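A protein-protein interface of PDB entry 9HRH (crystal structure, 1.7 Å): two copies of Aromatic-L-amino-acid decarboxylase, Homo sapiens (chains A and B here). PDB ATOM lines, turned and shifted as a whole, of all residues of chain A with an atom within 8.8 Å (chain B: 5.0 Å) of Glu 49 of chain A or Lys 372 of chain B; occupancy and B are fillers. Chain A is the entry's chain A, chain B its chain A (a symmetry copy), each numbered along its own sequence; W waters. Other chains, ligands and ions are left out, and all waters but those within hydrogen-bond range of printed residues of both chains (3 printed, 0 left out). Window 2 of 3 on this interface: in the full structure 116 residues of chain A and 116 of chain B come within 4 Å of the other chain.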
ATOM      1  N   ALA A  45       2.944 -25.667 -14.520  1.00  0.00           N
ATOM      2  CA  ALA A  45       1.789 -24.989 -15.091  1.00  0.00           C
ATOM      3  C   ALA A  45       0.517 -25.726 -14.702  1.00  0.00           C
ATOM      4  O   ALA A  45       0.535 -26.918 -14.381  1.00  0.00           O
ATOM      5  CB  ALA A  45       1.892 -24.885 -16.618  1.00  0.00           C
ATOM      6  N   ALA A  46      -0.595 -24.995 -14.733  1.00  0.00           N
ATOM      7  CA  ALA A  46      -1.885 -25.582 -14.416  1.00  0.00           C
ATOM      8  C   ALA A  46      -2.250 -26.642 -15.452  1.00  0.00           C
ATOM      9  O   ALA A  46      -1.873 -26.536 -16.623  1.00  0.00           O
ATOM     10  CB  ALA A  46      -2.967 -24.505 -14.366  1.00  0.00           C
ATOM     11  N   PRO A  47      -2.977 -27.683 -15.048  1.00  0.00           N
ATOM     12  CA  PRO A  47      -3.381 -28.710 -16.012  1.00  0.00           C
ATOM     13  C   PRO A  47      -4.420 -28.171 -16.982  1.00  0.00           C
ATOM     14  O   PRO A  47      -5.298 -27.388 -16.609  1.00  0.00           O
ATOM     15  CB  PRO A  47      -3.959 -29.812 -15.120  1.00  0.00           C
ATOM     16  CG  PRO A  47      -4.515 -29.035 -13.960  1.00  0.00           C
ATOM     17  CD  PRO A  47      -3.431 -28.024 -13.689  1.00  0.00           C
ATOM     18  N   GLN A  48      -4.309 -28.595 -18.240  1.00  0.00           N
ATOM     19  CA  GLN A  48      -5.278 -28.166 -19.243  1.00  0.00           C
ATOM     20  C   GLN A  48      -6.588 -28.937 -19.106  1.00  0.00           C
ATOM     21  O   GLN A  48      -7.670 -28.357 -19.250  1.00  0.00           O
ATOM     22  CB  GLN A  48      -4.688 -28.335 -20.645  1.00  0.00           C
ATOM     23  CG  GLN A  48      -3.596 -27.321 -20.967  1.00  0.00           C
ATOM     24  CD  GLN A  48      -4.142 -25.949 -21.311  1.00  0.00           C
ATOM     25  OE1 GLN A  48      -5.137 -25.824 -22.025  1.00  0.00           O
ATOM     26  NE2 GLN A  48      -3.494 -24.910 -20.797  1.00  0.00           N
ATOM     27  N   GLU A  49      -6.506 -30.265 -18.817  1.00  0.00           N
ATOM     28  CA  GLU A  49      -7.586 -31.180 -18.486  1.00  0.00           C
ATOM     29  C   GLU A  49      -7.713 -31.316 -16.971  1.00  0.00           C
ATOM     30  O   GLU A  49      -6.728 -31.164 -16.243  1.00  0.00           O
ATOM     31  CB  GLU A  49      -7.338 -32.561 -19.106  1.00  0.00           C
ATOM     32  CG  GLU A  49      -7.197 -32.578 -20.636  1.00  0.00           C
ATOM     33  CD  GLU A  49      -8.441 -32.095 -21.377  1.00  0.00           C
ATOM     34  OE1 GLU A  49      -9.533 -32.091 -20.773  1.00  0.00           O
ATOM     35  OE2 GLU A  49      -8.332 -31.721 -22.568  1.00  0.00           O
ATOM     36  N   PRO A  50      -8.914 -31.591 -16.463  1.00  0.00           N
ATOM     37  CA  PRO A  50      -9.091 -31.705 -15.012  1.00  0.00           C
ATOM     38  C   PRO A  50      -8.340 -32.888 -14.416  1.00  0.00           C
ATOM     39  O   PRO A  50      -8.201 -33.950 -15.030  1.00  0.00           O
ATOM     40  CB  PRO A  50     -10.609 -31.876 -14.859  1.00  0.00           C
ATOM     41  CG  PRO A  50     -11.174 -31.279 -16.119  1.00  0.00           C
ATOM     42  CD  PRO A  50     -10.200 -31.718 -17.166  1.00  0.00           C
ATOM     43  N   ASP A  51      -7.833 -32.675 -13.206  1.00  0.00           N
ATOM     44  CA  ASP A  51      -7.299 -33.740 -12.374  1.00  0.00           C
ATOM     45  C   ASP A  51      -8.432 -34.372 -11.571  1.00  0.00           C
ATOM     46  O   ASP A  51      -9.516 -33.801 -11.428  1.00  0.00           O
ATOM     47  CB  ASP A  51      -6.217 -33.202 -11.431  1.00  0.00           C
ATOM     48  CG  ASP A  51      -4.889 -32.953 -12.131  1.00  0.00           C
ATOM     49  OD1 ASP A  51      -4.669 -33.524 -13.219  1.00  0.00           O
ATOM     50  OD2 ASP A  51      -4.062 -32.186 -11.589  1.00  0.00           O
ATOM     51  N   THR A  52      -8.175 -35.565 -11.045  1.00  0.00           N
ATOM     52  CA  THR A  52      -9.171 -36.254 -10.236  1.00  0.00           C
ATOM     53  C   THR A  52      -9.082 -35.809  -8.780  1.00  0.00           C
ATOM     54  O   THR A  52      -8.024 -35.401  -8.295  1.00  0.00           O
ATOM     55  CB  THR A  52      -8.998 -37.774 -10.316  1.00  0.00           C
ATOM     56  OG1 THR A  52      -7.766 -38.153  -9.693  1.00  0.00           O
ATOM     57  CG2 THR A  52      -8.991 -38.243 -11.766  1.00  0.00           C
ATOM     58  N   ASP A  55      -6.506 -37.813  -7.016  1.00  0.00           N
ATOM     59  CA  ASP A  55      -5.152 -37.314  -7.231  1.00  0.00           C
ATOM     60  C   ASP A  55      -4.851 -36.131  -6.320  1.00  0.00           C
ATOM     61  O   ASP A  55      -3.748 -36.022  -5.772  1.00  0.00           O
ATOM     62  CB  ASP A  55      -4.982 -36.926  -8.701  1.00  0.00           C
ATOM     63  CG  ASP A  55      -3.558 -36.555  -9.050  1.00  0.00           C
ATOM     64  OD1 ASP A  55      -2.641 -36.927  -8.291  1.00  0.00           O
ATOM     65  OD2 ASP A  55      -3.355 -35.891 -10.087  1.00  0.00           O
ATOM     66  N   ARG B 367      -7.173 -27.268 -10.676  1.00  0.00           N
ATOM     67  CA  ARG B 367      -6.955 -28.676 -10.991  1.00  0.00           C
ATOM     68  C   ARG B 367      -8.252 -29.396 -11.341  1.00  0.00           C
ATOM     69  O   ARG B 367      -8.257 -30.263 -12.218  1.00  0.00           O
ATOM     70  CB  ARG B 367      -6.260 -29.376  -9.822  1.00  0.00           C
ATOM     71  CG  ARG B 367      -4.829 -28.914  -9.584  1.00  0.00           C
ATOM     72  CD  ARG B 367      -4.121 -29.778  -8.547  1.00  0.00           C
ATOM     73  NE  ARG B 367      -3.938 -31.156  -8.983  1.00  0.00           N
ATOM     74  CZ  ARG B 367      -3.366 -32.101  -8.249  1.00  0.00           C
ATOM     75  NH1 ARG B 367      -2.931 -31.855  -7.025  1.00  0.00           N
ATOM     76  NH2 ARG B 367      -3.228 -33.324  -8.755  1.00  0.00           N
ATOM     77  N   TYR B 369     -11.101 -28.061 -12.543  1.00  0.00           N
ATOM     78  CA  TYR B 369     -11.652 -27.539 -13.784  1.00  0.00           C
ATOM     79  C   TYR B 369     -10.690 -27.652 -14.953  1.00  0.00           C
ATOM     80  O   TYR B 369     -11.127 -27.914 -16.078  1.00  0.00           O
ATOM     81  CB  TYR B 369     -12.056 -26.074 -13.617  1.00  0.00           C
ATOM     82  CG  TYR B 369     -13.433 -25.893 -13.030  1.00  0.00           C
ATOM     83  CD1 TYR B 369     -14.563 -25.942 -13.836  1.00  0.00           C
ATOM     84  CD2 TYR B 369     -13.605 -25.695 -11.669  1.00  0.00           C
ATOM     85  CE1 TYR B 369     -15.827 -25.780 -13.303  1.00  0.00           C
ATOM     86  CE2 TYR B 369     -14.861 -25.536 -11.127  1.00  0.00           C
ATOM     87  CZ  TYR B 369     -15.970 -25.578 -11.947  1.00  0.00           C
ATOM     88  OH  TYR B 369     -17.226 -25.419 -11.404  1.00  0.00           O
ATOM     89  N   GLY B 370      -9.394 -27.465 -14.721  1.00  0.00           N
ATOM     90  CA  GLY B 370      -8.448 -27.382 -15.812  1.00  0.00           C
ATOM     91  C   GLY B 370      -8.508 -26.014 -16.461  1.00  0.00           C
ATOM     92  O   GLY B 370      -9.523 -25.317 -16.330  1.00  0.00           O
ATOM     93  N   VAL B 371      -7.455 -25.624 -17.185  1.00  0.00           N
ATOM     94  CA  VAL B 371      -7.489 -24.341 -17.883  1.00  0.00           C
ATOM     95  C   VAL B 371      -8.641 -24.312 -18.880  1.00  0.00           C
ATOM     96  O   VAL B 371      -9.344 -23.302 -19.013  1.00  0.00           O
ATOM     97  CB  VAL B 371      -6.138 -24.063 -18.564  1.00  0.00           C
ATOM     98  CG1 VAL B 371      -6.201 -22.778 -19.368  1.00  0.00           C
ATOM     99  CG2 VAL B 371      -5.021 -23.982 -17.528  1.00  0.00           C
ATOM    100  N   LYS B 372      -8.866 -25.426 -19.575  1.00  0.00           N
ATOM    101  CA  LYS B 372      -9.924 -25.476 -20.576  1.00  0.00           C
ATOM    102  C   LYS B 372     -11.307 -25.378 -19.943  1.00  0.00           C
ATOM    103  O   LYS B 372     -12.222 -24.806 -20.546  1.00  0.00           O
ATOM    104  CB  LYS B 372      -9.799 -26.756 -21.401  1.00  0.00           C
ATOM    105  CG  LYS B 372      -8.619 -26.740 -22.356  1.00  0.00           C
ATOM    106  CD  LYS B 372      -8.438 -28.072 -23.059  1.00  0.00           C
ATOM    107  CE  LYS B 372      -7.118 -28.108 -23.812  1.00  0.00           C
ATOM    108  NZ  LYS B 372      -7.304 -28.501 -25.235  1.00  0.00           N
ATOM    109  N   GLY B 373     -11.480 -25.928 -18.739  1.00  0.00           N
ATOM    110  CA  GLY B 373     -12.754 -25.789 -18.057  1.00  0.00           C
ATOM    111  C   GLY B 373     -13.043 -24.354 -17.660  1.00  0.00           C
ATOM    112  O   GLY B 373     -14.176 -23.879 -17.785  1.00  0.00           O
ATOM    113  N   LEU B 374     -12.022 -23.641 -17.179  1.00  0.00           N
ATOM    114  CA  LEU B 374     -12.199 -22.235 -16.833  1.00  0.00           C
ATOM    115  C   LEU B 374     -12.439 -21.388 -18.075  1.00  0.00           C
ATOM    116  O   LEU B 374     -13.240 -20.446 -18.045  1.00  0.00           O
ATOM    117  CB  LEU B 374     -10.979 -21.730 -16.060  1.00  0.00           C
ATOM    118  CG  LEU B 374     -10.721 -22.389 -14.703  1.00  0.00           C
ATOM    119  CD1 LEU B 374      -9.464 -21.827 -14.052  1.00  0.00           C
ATOM    120  CD2 LEU B 374     -11.924 -22.214 -13.790  1.00  0.00           C
ATOM    121  N   GLN B 375     -11.756 -21.707 -19.179  1.00  0.00           N
ATOM    122  CA  GLN B 375     -11.978 -20.972 -20.421  1.00  0.00           C
ATOM    123  C   GLN B 375     -13.401 -21.165 -20.928  1.00  0.00           C
ATOM    124  O   GLN B 375     -14.029 -20.216 -21.410  1.00  0.00           O
ATOM    125  CB  GLN B 375     -10.969 -21.408 -21.485  1.00  0.00           C
ATOM    126  CG  GLN B 375      -9.547 -20.917 -21.254  1.00  0.00           C
ATOM    127  CD  GLN B 375      -8.549 -21.535 -22.221  1.00  0.00           C
ATOM    128  OE1 GLN B 375      -8.665 -22.703 -22.593  1.00  0.00           O
ATOM    129  NE2 GLN B 375      -7.563 -20.748 -22.636  1.00  0.00           N
ATOM    130  N   ALA B 376     -13.926 -22.389 -20.828  1.00  0.00           N
ATOM    131  CA  ALA B 376     -15.298 -22.640 -21.257  1.00  0.00           C
ATOM    132  C   ALA B 376     -16.294 -21.883 -20.387  1.00  0.00           C
ATOM    133  O   ALA B 376     -17.330 -21.416 -20.875  1.00  0.00           O
ATOM    134  CB  ALA B 376     -15.591 -24.140 -21.233  1.00  0.00           C
HETATM  135  O   HOH W   1      -6.505 -23.990 -23.570  1.00  0.00           O
HETATM  136  O   HOH W   2      -1.722 -30.548 -11.405  1.00  0.00           O
HETATM  137  O   HOH W   3     -10.317 -28.677 -18.604  1.00  0.00           O
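No position is printed for both chains.
Hydrophobic or aromatic side chains of chain B within 4 Å of the printed part of chain A: Val 371. Along chain B the printed residues that touch a printed residue of chain A span positions 367 to 372. Hydrophobic or aromatic side chains of chain A within 4 Å of the printed part of chain B: Ala 46, Pro 47 and Pro 50. Among the printed residues, Asp or Glu carboxylates within 4 Å of a Lys or Arg side-chain nitrogen of the other chain: Asp 51 of chain A with Arg 367 of chain B and Asp 55 of chain A with Arg 367 of chain B.
The side-chain hydroxyl of Thr 52 of chain A is in hydrogen-bond range of the backbone NH of Asp 55 of chain A (3.0 Å).
Water W1 bridges OE1 of Gln 375 of chain B (2.7 Å) and OE1 of Gln 48 of chain A (2.8 Å). Water W3 lies within hydrogen-bond range of the backbone carbonyl oxygen of Gln 48 of chain A (2.7 Å), the backbone carbonyl oxygen of Tyr 369 of chain B (2.8 Å) and the backbone NH of Gly 373 of chain B (3.0 Å). Water W2 lies within hydrogen-bond range of the side-chain carboxylate (OD2) of Asp 51 of chain A (2.9 Å) and the guanidinium group (NE) of Arg 367 of chain B (3.3 Å).
N of Val 371 of chain B sits at hydrogen-bond distance from O of Gln 48 of chain A, at 3.4 Å. OD2 of Asp 51 of chain A lies within salt-bridge range of NE of Arg 367 of chain B (2.8 Å). The backbone carbonyl oxygen (O) of Pro 47 of chain A is in hydrogen-bond range of the backbone NH (N) of Val 371 of chain B (2.8 Å). O of Gln 48 of chain A is in hydrogen-bond range of N of Lys 372 of chain B (3.2 Å). The side-chain carboxylate (OD2) of Asp 55 of chain A is in salt-bridge range of the guanidinium group (NH2) of Arg 367 of chain B (2.9 Å).
Among the printed residues, pairs that only touch across the chains: Ala 46 of chain A with Val 371 of chain B, Pro 47 of chain A with Arg 367 of chain B, Pro 47 of chain A with Gly 370 of chain B, Gln 48 of chain A with Gly 370 of chain B, Glu 49 of chain A with Lys 372 of chain B, Pro 50 of chain A with Arg 367 of chain B and Pro 50 of chain A with Tyr 369 of chain B.
Of chain B, only Lys 372 comes within 4 Å of Glu 49 of chain A. Printed residues of chain B within 4 Å of Asp 55 of chain A: Arg 367. Of the printed residues of chain A, Tyr 369 of chain B touches Pro 50. Of the printed residues of chain A, Gly 370 of chain B touches Pro 47 (3.2 Å) and Gln 48 (3.7 Å). Of chain A, only Ala 46 (3.8 Å), Pro 47 (2.8 Å) and Gln 48 (3.4 Å) come within 4 Å of Val 371 of chain B. Of chain A, only Gln 48 and Glu 49 come within 4 Å of Lys 372 of chain B. Gln 375 of chain B touches none of the printed residues of chain A. Ala 376 of chain B touches none of the printed residues of chain A. The nearest residue of chain B that does not touch Glu 49 of chain A is Gly 370 of chain B (4.2 Å). The nearest printed residue of chain B that does not touch Pro 47 of chain A is Lys 372 of chain B (5.0 Å).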
